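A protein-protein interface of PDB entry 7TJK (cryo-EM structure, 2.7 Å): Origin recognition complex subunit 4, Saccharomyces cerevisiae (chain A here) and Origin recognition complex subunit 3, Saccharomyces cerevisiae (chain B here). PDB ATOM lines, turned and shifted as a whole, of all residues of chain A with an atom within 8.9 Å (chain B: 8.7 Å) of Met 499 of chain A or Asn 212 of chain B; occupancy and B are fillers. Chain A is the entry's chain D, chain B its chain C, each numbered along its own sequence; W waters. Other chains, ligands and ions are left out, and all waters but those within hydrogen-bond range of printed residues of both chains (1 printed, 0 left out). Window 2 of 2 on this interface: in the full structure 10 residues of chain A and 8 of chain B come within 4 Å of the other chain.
The backbone carbonyl oxygen of Pro 137 of chain B sits at hydrogen-bond distance from the side-chain amide nitrogen of Gln 494 of chain A, at 3.4 Å. The side-chain hydroxyl (OG1) of Thr 498 of chain A sits at hydrogen-bond distance from the side-chain amide nitrogen (ND2) of Asn 212 of chain B (3.2 Å).
N of Asn 214 of chain B sits close to OD1 of Asn 212 of chain B, at 3.4 Å. The backbone carbonyl oxygen of Phe 495 of chain A lies within hydrogen-bond range of the side-chain hydroxyl of Thr 498 of chain A (2.8 Å).
Gln 494 of chain A touches Asn 212 of chain B. Asn 212 of chain B touches Met 499 of chain A.
Printed residues of chain B within 4 Å of Thr 498 of chain A: Asn 212. Met 499 of chain A touches one residue of chain B. Printed residues of chain A within 4 Å of Pro 137 of chain B: Gln 494 (3.4 Å). No residue of chain A comes within 4 Å of Ile 211 of chain B. Of chain A, only Gln 494, Thr 498 and Met 499 come within 4 Å of Asn 212 of chain B. The nearest printed residue of chain B that does not touch Gln 494 of chain A is Thr 215 of chain B (4.4 Å).
Of the 12 printed residues of chain A, 3 touch a printed residue of chain B. Printed residues of chain B that touch a printed residue of chain A: Pro 137 and Asn 212. Among the printed residues, 4 pairs touch across the chains. Among the printed residues, no Asp or Glu carboxylate lies within 4 Å of a Lys or Arg side-chain nitrogen of the other chain.
Water W1 lies within hydrogen-bond range of the backbone carbonyl oxygen (O) of Thr 498 of chain A (2.8 Å) and the backbone NH (N) of Phe 213 of chain B (3.0 Å).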
ATOM      1  N   TYR A 493      -1.246  12.485  14.008  1.00  0.00           N
ATOM      2  CA  TYR A 493      -2.315  12.469  13.022  1.00  0.00           C
ATOM      3  C   TYR A 493      -3.652  12.454  13.746  1.00  0.00           C
ATOM      4  O   TYR A 493      -3.841  11.676  14.685  1.00  0.00           O
ATOM      5  CB  TYR A 493      -2.186  11.251  12.099  1.00  0.00           C
ATOM      6  CG  TYR A 493      -3.291  11.112  11.078  1.00  0.00           C
ATOM      7  CD1 TYR A 493      -3.292  11.878   9.920  1.00  0.00           C
ATOM      8  CD2 TYR A 493      -4.327  10.204  11.268  1.00  0.00           C
ATOM      9  CE1 TYR A 493      -4.296  11.749   8.983  1.00  0.00           C
ATOM     10  CE2 TYR A 493      -5.336  10.071  10.339  1.00  0.00           C
ATOM     11  CZ  TYR A 493      -5.314  10.843   9.198  1.00  0.00           C
ATOM     12  OH  TYR A 493      -6.319  10.708   8.270  1.00  0.00           O
ATOM     13  N   GLN A 494      -4.569  13.316  13.315  1.00  0.00           N
ATOM     14  CA  GLN A 494      -5.917  13.348  13.866  1.00  0.00           C
ATOM     15  C   GLN A 494      -6.794  12.391  13.069  1.00  0.00           C
ATOM     16  O   GLN A 494      -7.077  12.638  11.892  1.00  0.00           O
ATOM     17  CB  GLN A 494      -6.497  14.763  13.830  1.00  0.00           C
ATOM     18  CG  GLN A 494      -5.706  15.829  14.588  1.00  0.00           C
ATOM     19  CD  GLN A 494      -4.960  15.289  15.795  1.00  0.00           C
ATOM     20  OE1 GLN A 494      -5.565  14.924  16.804  1.00  0.00           O
ATOM     21  NE2 GLN A 494      -3.635  15.244  15.700  1.00  0.00           N
ATOM     22  N   PHE A 495      -7.220  11.308  13.708  1.00  0.00           N
ATOM     23  CA  PHE A 495      -8.057  10.319  13.051  1.00  0.00           C
ATOM     24  C   PHE A 495      -9.486  10.837  12.910  1.00  0.00           C
ATOM     25  O   PHE A 495      -9.962  11.651  13.706  1.00  0.00           O
ATOM     26  CB  PHE A 495      -8.033   9.002  13.828  1.00  0.00           C
ATOM     27  CG  PHE A 495      -6.741   8.246  13.693  1.00  0.00           C
ATOM     28  CD1 PHE A 495      -5.680   8.502  14.549  1.00  0.00           C
ATOM     29  CD2 PHE A 495      -6.584   7.288  12.704  1.00  0.00           C
ATOM     30  CE1 PHE A 495      -4.487   7.811  14.425  1.00  0.00           C
ATOM     31  CE2 PHE A 495      -5.396   6.593  12.575  1.00  0.00           C
ATOM     32  CZ  PHE A 495      -4.346   6.855  13.435  1.00  0.00           C
ATOM     33  N   GLN A 496     -10.173  10.347  11.872  1.00  0.00           N
ATOM     34  CA  GLN A 496     -11.506  10.851  11.554  1.00  0.00           C
ATOM     35  C   GLN A 496     -12.553  10.382  12.557  1.00  0.00           C
ATOM     36  O   GLN A 496     -13.597  11.025  12.703  1.00  0.00           O
ATOM     37  CB  GLN A 496     -11.909  10.428  10.142  1.00  0.00           C
ATOM     38  CG  GLN A 496     -11.166  11.159   9.038  1.00  0.00           C
ATOM     39  CD  GLN A 496     -11.424  12.652   9.041  1.00  0.00           C
ATOM     40  OE1 GLN A 496     -12.547  13.102   9.273  1.00  0.00           O
ATOM     41  NE2 GLN A 496     -10.382  13.430   8.775  1.00  0.00           N
ATOM     42  N   GLY A 497     -12.294   9.276  13.255  1.00  0.00           N
ATOM     43  CA  GLY A 497     -13.199   8.816  14.289  1.00  0.00           C
ATOM     44  C   GLY A 497     -13.205   9.665  15.545  1.00  0.00           C
ATOM     45  O   GLY A 497     -14.188   9.621  16.292  1.00  0.00           O
ATOM     46  N   THR A 498     -12.147  10.432  15.790  1.00  0.00           N
ATOM     47  CA  THR A 498     -12.051  11.266  16.982  1.00  0.00           C
ATOM     48  C   THR A 498     -12.614  12.667  16.780  1.00  0.00           C
ATOM     49  O   THR A 498     -12.574  13.471  17.715  1.00  0.00           O
ATOM     50  CB  THR A 498     -10.593  11.366  17.446  1.00  0.00           C
ATOM     51  OG1 THR A 498      -9.833  12.116  16.490  1.00  0.00           O
ATOM     52  CG2 THR A 498      -9.984   9.983  17.595  1.00  0.00           C
ATOM     53  N   MET A 499     -13.131  12.981  15.593  1.00  0.00           N
ATOM     54  CA  MET A 499     -13.680  14.301  15.318  1.00  0.00           C
ATOM     55  C   MET A 499     -15.179  14.295  15.057  1.00  0.00           C
ATOM     56  O   MET A 499     -15.786  15.370  15.021  1.00  0.00           O
ATOM     57  CB  MET A 499     -12.958  14.936  14.121  1.00  0.00           C
ATOM     58  CG  MET A 499     -11.529  15.354  14.420  1.00  0.00           C
ATOM     59  SD  MET A 499     -10.697  16.026  12.971  1.00  0.00           S
ATOM     60  CE  MET A 499     -10.423  14.534  12.026  1.00  0.00           C
ATOM     61  N   ILE A 500     -15.784  13.127  14.873  1.00  0.00           N
ATOM     62  CA  ILE A 500     -17.227  13.013  14.691  1.00  0.00           C
ATOM     63  C   ILE A 500     -17.838  12.725  16.059  1.00  0.00           C
ATOM     64  O   ILE A 500     -17.109  12.302  16.968  1.00  0.00           O
ATOM     65  CB  ILE A 500     -17.567  11.931  13.649  1.00  0.00           C
ATOM     66  CG1 ILE A 500     -17.266  10.536  14.192  1.00  0.00           C
ATOM     67  CG2 ILE A 500     -16.802  12.177  12.356  1.00  0.00           C
ATOM     68  CD1 ILE A 500     -17.843   9.437  13.351  1.00  0.00           C
ATOM     69  N   PRO A 501     -19.132  12.988  16.277  1.00  0.00           N
ATOM     70  CA  PRO A 501     -19.751  12.634  17.560  1.00  0.00           C
ATOM     71  C   PRO A 501     -19.783  11.131  17.792  1.00  0.00           C
ATOM     72  O   PRO A 501     -19.781  10.329  16.855  1.00  0.00           O
ATOM     73  CB  PRO A 501     -21.170  13.210  17.448  1.00  0.00           C
ATOM     74  CG  PRO A 501     -21.362  13.529  15.998  1.00  0.00           C
ATOM     75  CD  PRO A 501     -20.006  13.880  15.495  1.00  0.00           C
ATOM     76  N   PHE A 502     -19.801  10.762  19.079  1.00  0.00           N
ATOM     77  CA  PHE A 502     -19.642   9.374  19.503  1.00  0.00           C
ATOM     78  C   PHE A 502     -20.789   8.478  19.052  1.00  0.00           C
ATOM     79  O   PHE A 502     -20.598   7.264  18.938  1.00  0.00           O
ATOM     80  CB  PHE A 502     -19.498   9.305  21.029  1.00  0.00           C
ATOM     81  CG  PHE A 502     -20.812   9.254  21.766  1.00  0.00           C
ATOM     82  CD1 PHE A 502     -21.591  10.392  21.891  1.00  0.00           C
ATOM     83  CD2 PHE A 502     -21.259   8.072  22.345  1.00  0.00           C
ATOM     84  CE1 PHE A 502     -22.800  10.352  22.566  1.00  0.00           C
ATOM     85  CE2 PHE A 502     -22.467   8.026  23.014  1.00  0.00           C
ATOM     86  CZ  PHE A 502     -23.235   9.167  23.127  1.00  0.00           C
ATOM     87  N   LEU A 504     -22.038   8.391  16.146  1.00  0.00           N
ATOM     88  CA  LEU A 504     -21.841   8.050  14.747  1.00  0.00           C
ATOM     89  C   LEU A 504     -20.553   7.285  14.481  1.00  0.00           C
ATOM     90  O   LEU A 504     -20.291   6.940  13.323  1.00  0.00           O
ATOM     91  CB  LEU A 504     -21.863   9.320  13.883  1.00  0.00           C
ATOM     92  CG  LEU A 504     -23.215  10.005  13.681  1.00  0.00           C
ATOM     93  CD1 LEU A 504     -23.120  11.084  12.614  1.00  0.00           C
ATOM     94  CD2 LEU A 504     -24.282   8.994  13.316  1.00  0.00           C
ATOM     95  N   ARG A 505     -19.741   7.019  15.502  1.00  0.00           N
ATOM     96  CA  ARG A 505     -18.512   6.258  15.308  1.00  0.00           C
ATOM     97  C   ARG A 505     -18.829   4.802  14.999  1.00  0.00           C
ATOM     98  O   ARG A 505     -19.658   4.179  15.668  1.00  0.00           O
ATOM     99  CB  ARG A 505     -17.621   6.348  16.545  1.00  0.00           C
ATOM    100  CG  ARG A 505     -17.099   7.736  16.847  1.00  0.00           C
ATOM    101  CD  ARG A 505     -16.317   7.756  18.149  1.00  0.00           C
ATOM    102  NE  ARG A 505     -16.028   9.117  18.583  1.00  0.00           N
ATOM    103  CZ  ARG A 505     -15.867   9.483  19.847  1.00  0.00           C
ATOM    104  NH1 ARG A 505     -15.941   8.606  20.835  1.00  0.00           N
ATOM    105  NH2 ARG A 505     -15.631  10.761  20.127  1.00  0.00           N
ATOM    106  N   THR B 132      -3.792  26.453  23.336  1.00  0.00           N
ATOM    107  CA  THR B 132      -4.223  26.591  21.951  1.00  0.00           C
ATOM    108  C   THR B 132      -4.352  25.201  21.320  1.00  0.00           C
ATOM    109  O   THR B 132      -3.557  24.311  21.635  1.00  0.00           O
ATOM    110  CB  THR B 132      -3.207  27.443  21.176  1.00  0.00           C
ATOM    111  OG1 THR B 132      -3.123  28.739  21.780  1.00  0.00           O
ATOM    112  CG2 THR B 132      -3.579  27.628  19.711  1.00  0.00           C
ATOM    113  N   PRO B 133      -5.370  24.951  20.482  1.00  0.00           N
ATOM    114  CA  PRO B 133      -5.429  23.663  19.761  1.00  0.00           C
ATOM    115  C   PRO B 133      -4.256  23.419  18.824  1.00  0.00           C
ATOM    116  O   PRO B 133      -3.923  22.255  18.562  1.00  0.00           O
ATOM    117  CB  PRO B 133      -6.754  23.750  18.985  1.00  0.00           C
ATOM    118  CG  PRO B 133      -7.191  25.178  19.082  1.00  0.00           C
ATOM    119  CD  PRO B 133      -6.623  25.707  20.345  1.00  0.00           C
ATOM    120  N   LYS B 134      -3.626  24.476  18.301  1.00  0.00           N
ATOM    121  CA  LYS B 134      -2.385  24.314  17.549  1.00  0.00           C
ATOM    122  C   LYS B 134      -1.255  23.834  18.454  1.00  0.00           C
ATOM    123  O   LYS B 134      -0.409  23.041  18.026  1.00  0.00           O
ATOM    124  CB  LYS B 134      -2.024  25.635  16.860  1.00  0.00           C
ATOM    125  CG  LYS B 134      -0.686  25.661  16.129  1.00  0.00           C
ATOM    126  CD  LYS B 134      -0.768  24.977  14.773  1.00  0.00           C
ATOM    127  CE  LYS B 134      -1.110  25.969  13.674  1.00  0.00           C
ATOM    128  NZ  LYS B 134      -1.212  25.312  12.341  1.00  0.00           N
ATOM    129  N   SER B 136      -1.781  21.836  20.864  1.00  0.00           N
ATOM    130  CA  SER B 136      -2.270  20.573  21.414  1.00  0.00           C
ATOM    131  C   SER B 136      -2.485  19.528  20.321  1.00  0.00           C
ATOM    132  O   SER B 136      -3.627  19.146  20.041  1.00  0.00           O
ATOM    133  CB  SER B 136      -3.571  20.810  22.180  1.00  0.00           C
ATOM    134  OG  SER B 136      -3.439  21.888  23.089  1.00  0.00           O
ATOM    135  N   PRO B 137      -1.401  19.012  19.685  1.00  0.00           N
ATOM    136  CA  PRO B 137      -1.607  17.925  18.718  1.00  0.00           C
ATOM    137  C   PRO B 137      -1.826  16.578  19.394  1.00  0.00           C
ATOM    138  O   PRO B 137      -2.482  15.696  18.835  1.00  0.00           O
ATOM    139  CB  PRO B 137      -0.319  17.945  17.889  1.00  0.00           C
ATOM    140  CG  PRO B 137       0.707  18.452  18.810  1.00  0.00           C
ATOM    141  CD  PRO B 137       0.027  19.380  19.777  1.00  0.00           C
ATOM    142  N   ASN B 138      -1.281  16.416  20.598  1.00  0.00           N
ATOM    143  CA  ASN B 138      -1.434  15.198  21.380  1.00  0.00           C
ATOM    144  C   ASN B 138      -1.216  15.552  22.844  1.00  0.00           C
ATOM    145  O   ASN B 138      -0.893  16.690  23.186  1.00  0.00           O
ATOM    146  CB  ASN B 138      -0.474  14.092  20.915  1.00  0.00           C
ATOM    147  CG  ASN B 138       0.944  14.592  20.703  1.00  0.00           C
ATOM    148  OD1 ASN B 138       1.647  14.930  21.652  1.00  0.00           O
ATOM    149  ND2 ASN B 138       1.374  14.629  19.447  1.00  0.00           N
ATOM    150  N   VAL B 139      -1.416  14.553  23.708  1.00  0.00           N
ATOM    151  CA  VAL B 139      -1.322  14.759  25.151  1.00  0.00           C
ATOM    152  C   VAL B 139       0.116  15.023  25.582  1.00  0.00           C
ATOM    153  O   VAL B 139       0.362  15.805  26.513  1.00  0.00           O
ATOM    154  CB  VAL B 139      -1.923  13.543  25.878  1.00  0.00           C
ATOM    155  CG1 VAL B 139      -2.124  13.835  27.350  1.00  0.00           C
ATOM    156  CG2 VAL B 139      -3.231  13.156  25.231  1.00  0.00           C
ATOM    157  N   MET B 142       1.048  18.603  24.998  1.00  0.00           N
ATOM    158  CA  MET B 142       0.339  19.412  25.986  1.00  0.00           C
ATOM    159  C   MET B 142       1.068  19.416  27.320  1.00  0.00           C
ATOM    160  O   MET B 142       1.305  20.481  27.908  1.00  0.00           O
ATOM    161  CB  MET B 142      -1.082  18.882  26.167  1.00  0.00           C
ATOM    162  CG  MET B 142      -2.078  19.432  25.185  1.00  0.00           C
ATOM    163  SD  MET B 142      -3.725  18.719  25.350  1.00  0.00           S
ATOM    164  CE  MET B 142      -4.607  20.049  26.156  1.00  0.00           C
ATOM    165  N   ASP B 207     -10.068  28.417  22.816  1.00  0.00           N
ATOM    166  CA  ASP B 207     -10.837  27.862  21.700  1.00  0.00           C
ATOM    167  C   ASP B 207     -11.116  26.369  21.843  1.00  0.00           C
ATOM    168  O   ASP B 207     -10.624  25.567  21.042  1.00  0.00           O
ATOM    169  CB  ASP B 207     -10.113  28.128  20.375  1.00  0.00           C
ATOM    170  CG  ASP B 207     -10.104  29.590  19.998  1.00  0.00           C
ATOM    171  OD1 ASP B 207     -11.048  30.313  20.381  1.00  0.00           O
ATOM    172  OD2 ASP B 207      -9.151  30.021  19.318  1.00  0.00           O
ATOM    173  N   VAL B 208     -11.896  25.991  22.861  1.00  0.00           N
ATOM    174  CA  VAL B 208     -12.119  24.583  23.175  1.00  0.00           C
ATOM    175  C   VAL B 208     -12.959  23.885  22.107  1.00  0.00           C
ATOM    176  O   VAL B 208     -12.828  22.670  21.914  1.00  0.00           O
ATOM    177  CB  VAL B 208     -12.762  24.472  24.574  1.00  0.00           C
ATOM    178  CG1 VAL B 208     -12.738  23.041  25.102  1.00  0.00           C
ATOM    179  CG2 VAL B 208     -12.053  25.384  25.543  1.00  0.00           C
ATOM    180  N   ASP B 209     -13.793  24.630  21.378  1.00  0.00           N
ATOM    181  CA  ASP B 209     -14.623  24.039  20.334  1.00  0.00           C
ATOM    182  C   ASP B 209     -13.807  23.517  19.155  1.00  0.00           C
ATOM    183  O   ASP B 209     -14.276  22.623  18.444  1.00  0.00           O
ATOM    184  CB  ASP B 209     -15.649  25.063  19.844  1.00  0.00           C
ATOM    185  CG  ASP B 209     -16.699  25.380  20.889  1.00  0.00           C
ATOM    186  OD1 ASP B 209     -17.000  24.497  21.720  1.00  0.00           O
ATOM    187  OD2 ASP B 209     -17.225  26.511  20.883  1.00  0.00           O
ATOM    188  N   SER B 210     -12.599  24.040  18.943  1.00  0.00           N
ATOM    189  CA  SER B 210     -11.735  23.611  17.853  1.00  0.00           C
ATOM    190  C   SER B 210     -10.720  22.548  18.255  1.00  0.00           C
ATOM    191  O   SER B 210     -10.017  22.030  17.381  1.00  0.00           O
ATOM    192  CB  SER B 210     -10.988  24.817  17.268  1.00  0.00           C
ATOM    193  OG  SER B 210     -10.333  24.474  16.061  1.00  0.00           O
ATOM    194  N   ILE B 211     -10.622  22.208  19.535  1.00  0.00           N
ATOM    195  CA  ILE B 211      -9.631  21.234  19.979  1.00  0.00           C
ATOM    196  C   ILE B 211     -10.146  19.827  19.699  1.00  0.00           C
ATOM    197  O   ILE B 211     -11.350  19.602  19.518  1.00  0.00           O
ATOM    198  CB  ILE B 211      -9.288  21.438  21.474  1.00  0.00           C
ATOM    199  CG1 ILE B 211      -7.846  21.017  21.767  1.00  0.00           C
ATOM    200  CG2 ILE B 211     -10.233  20.664  22.386  1.00  0.00           C
ATOM    201  CD1 ILE B 211      -7.393  21.321  23.173  1.00  0.00           C
ATOM    202  N   ASN B 212      -9.221  18.875  19.618  1.00  0.00           N
ATOM    203  CA  ASN B 212      -9.598  17.470  19.581  1.00  0.00           C
ATOM    204  C   ASN B 212     -10.013  17.031  20.977  1.00  0.00           C
ATOM    205  O   ASN B 212      -9.208  17.077  21.914  1.00  0.00           O
ATOM    206  CB  ASN B 212      -8.439  16.620  19.070  1.00  0.00           C
ATOM    207  CG  ASN B 212      -8.887  15.255  18.605  1.00  0.00           C
ATOM    208  OD1 ASN B 212      -8.954  14.311  19.390  1.00  0.00           O
ATOM    209  ND2 ASN B 212      -9.201  15.142  17.322  1.00  0.00           N
ATOM    210  N   PHE B 213     -11.267  16.604  21.119  1.00  0.00           N
ATOM    211  CA  PHE B 213     -11.810  16.347  22.446  1.00  0.00           C
ATOM    212  C   PHE B 213     -11.284  15.058  23.061  1.00  0.00           C
ATOM    213  O   PHE B 213     -11.312  14.922  24.287  1.00  0.00           O
ATOM    214  CB  PHE B 213     -13.337  16.342  22.391  1.00  0.00           C
ATOM    215  CG  PHE B 213     -13.940  17.708  22.545  1.00  0.00           C
ATOM    216  CD1 PHE B 213     -14.125  18.259  23.805  1.00  0.00           C
ATOM    217  CD2 PHE B 213     -14.295  18.454  21.433  1.00  0.00           C
ATOM    218  CE1 PHE B 213     -14.669  19.522  23.954  1.00  0.00           C
ATOM    219  CE2 PHE B 213     -14.840  19.719  21.573  1.00  0.00           C
ATOM    220  CZ  PHE B 213     -15.027  20.251  22.837  1.00  0.00           C
ATOM    221  N   ASN B 214     -10.792  14.120  22.248  1.00  0.00           N
ATOM    222  CA  ASN B 214     -10.112  12.952  22.800  1.00  0.00           C
ATOM    223  C   ASN B 214      -8.795  13.343  23.460  1.00  0.00           C
ATOM    224  O   ASN B 214      -8.483  12.871  24.560  1.00  0.00           O
ATOM    225  CB  ASN B 214      -9.880  11.915  21.701  1.00  0.00           C
ATOM    226  CG  ASN B 214      -9.310  10.618  22.237  1.00  0.00           C
ATOM    227  OD1 ASN B 214      -9.889   9.990  23.122  1.00  0.00           O
ATOM    228  ND2 ASN B 214      -8.166  10.209  21.702  1.00  0.00           N
ATOM    229  N   THR B 215      -8.021  14.214  22.802  1.00  0.00           N
ATOM    230  CA  THR B 215      -6.760  14.700  23.358  1.00  0.00           C
ATOM    231  C   THR B 215      -6.987  15.504  24.635  1.00  0.00           C
ATOM    232  O   THR B 215      -6.279  15.310  25.633  1.00  0.00           O
ATOM    233  CB  THR B 215      -6.029  15.538  22.304  1.00  0.00           C
ATOM    234  OG1 THR B 215      -5.670  14.706  21.194  1.00  0.00           O
ATOM    235  CG2 THR B 215      -4.772  16.173  22.868  1.00  0.00           C
ATOM    236  N   LEU B 216      -8.000  16.379  24.633  1.00  0.00           N
ATOM    237  CA  LEU B 216      -8.341  17.155  25.823  1.00  0.00           C
ATOM    238  C   LEU B 216      -8.825  16.259  26.955  1.00  0.00           C
ATOM    239  O   LEU B 216      -8.459  16.470  28.118  1.00  0.00           O
ATOM    240  CB  LEU B 216      -9.405  18.197  25.482  1.00  0.00           C
ATOM    241  CG  LEU B 216      -9.876  19.067  26.651  1.00  0.00           C
ATOM    242  CD1 LEU B 216      -8.783  20.038  27.062  1.00  0.00           C
ATOM    243  CD2 LEU B 216     -11.159  19.798  26.310  1.00  0.00           C
ATOM    244  N   ASP B 217      -9.631  15.245  26.623  1.00  0.00           N
ATOM    245  CA  ASP B 217     -10.123  14.293  27.613  1.00  0.00           C
ATOM    246  C   ASP B 217      -8.976  13.531  28.272  1.00  0.00           C
ATOM    247  O   ASP B 217      -8.886  13.480  29.508  1.00  0.00           O
ATOM    248  CB  ASP B 217     -11.098  13.330  26.931  1.00  0.00           C
ATOM    249  CG  ASP B 217     -12.055  12.680  27.899  1.00  0.00           C
ATOM    250  OD1 ASP B 217     -11.928  12.922  29.109  1.00  0.00           O
ATOM    251  OD2 ASP B 217     -12.943  11.930  27.445  1.00  0.00           O
ATOM    252  N   ASN B 218      -8.061  12.989  27.460  1.00  0.00           N
ATOM    253  CA  ASN B 218      -6.915  12.262  27.997  1.00  0.00           C
ATOM    254  C   ASN B 218      -5.989  13.174  28.791  1.00  0.00           C
ATOM    255  O   ASN B 218      -5.409  12.738  29.790  1.00  0.00           O
ATOM    256  CB  ASN B 218      -6.154  11.572  26.867  1.00  0.00           C
ATOM    257  CG  ASN B 218      -7.010  10.574  26.110  1.00  0.00           C
ATOM    258  OD1 ASN B 218      -7.911   9.956  26.672  1.00  0.00           O
ATOM    259  ND2 ASN B 218      -6.732  10.417  24.822  1.00  0.00           N
ATOM    260  N   PHE B 219      -5.888  14.452  28.407  1.00  0.00           N
ATOM    261  CA  PHE B 219      -5.132  15.407  29.209  1.00  0.00           C
ATOM    262  C   PHE B 219      -5.809  15.686  30.551  1.00  0.00           C
ATOM    263  O   PHE B 219      -5.118  15.922  31.546  1.00  0.00           O
ATOM    264  CB  PHE B 219      -4.930  16.704  28.426  1.00  0.00           C
ATOM    265  CG  PHE B 219      -3.952  17.652  29.061  1.00  0.00           C
ATOM    266  CD1 PHE B 219      -2.604  17.327  29.133  1.00  0.00           C
ATOM    267  CD2 PHE B 219      -4.373  18.865  29.581  1.00  0.00           C
ATOM    268  CE1 PHE B 219      -1.695  18.194  29.717  1.00  0.00           C
ATOM    269  CE2 PHE B 219      -3.469  19.738  30.163  1.00  0.00           C
ATOM    270  CZ  PHE B 219      -2.129  19.400  30.231  1.00  0.00           C
ATOM    271  N   ILE B 220      -7.146  15.649  30.603  1.00  0.00           N
ATOM    272  CA  ILE B 220      -7.850  15.872  31.869  1.00  0.00           C
ATOM    273  C   ILE B 220      -7.643  14.701  32.833  1.00  0.00           C
ATOM    274  O   ILE B 220      -7.338  14.909  34.015  1.00  0.00           O
ATOM    275  CB  ILE B 220      -9.344  16.158  31.615  1.00  0.00           C
ATOM    276  CG1 ILE B 220      -9.527  17.539  30.987  1.00  0.00           C
ATOM    277  CG2 ILE B 220     -10.152  16.095  32.899  1.00  0.00           C
ATOM    278  CD1 ILE B 220     -10.874  17.735  30.333  1.00  0.00           C
ATOM    279  N   ASN B 250     -19.073  15.357  23.940  1.00  0.00           N
ATOM    280  CA  ASN B 250     -17.792  14.977  23.365  1.00  0.00           C
ATOM    281  C   ASN B 250     -16.818  14.435  24.398  1.00  0.00           C
ATOM    282  O   ASN B 250     -15.878  13.723  24.030  1.00  0.00           O
ATOM    283  CB  ASN B 250     -17.163  16.172  22.644  1.00  0.00           C
ATOM    284  CG  ASN B 250     -17.807  16.447  21.304  1.00  0.00           C
ATOM    285  OD1 ASN B 250     -17.378  15.919  20.278  1.00  0.00           O
ATOM    286  ND2 ASN B 250     -18.844  17.272  21.303  1.00  0.00           N
ATOM    287  N   LEU B 251     -17.010  14.763  25.670  1.00  0.00           N
ATOM    288  CA  LEU B 251     -16.231  14.177  26.746  1.00  0.00           C
ATOM    289  C   LEU B 251     -16.911  12.909  27.247  1.00  0.00           C
ATOM    290  O   LEU B 251     -18.108  12.694  27.045  1.00  0.00           O
ATOM    291  CB  LEU B 251     -16.058  15.168  27.898  1.00  0.00           C
ATOM    292  CG  LEU B 251     -15.313  16.478  27.630  1.00  0.00           C
ATOM    293  CD1 LEU B 251     -15.030  17.197  28.937  1.00  0.00           C
ATOM    294  CD2 LEU B 251     -14.023  16.236  26.867  1.00  0.00           C
HETATM  295  O   HOH W   1     -12.557  16.183  18.394  1.00  0.00           O
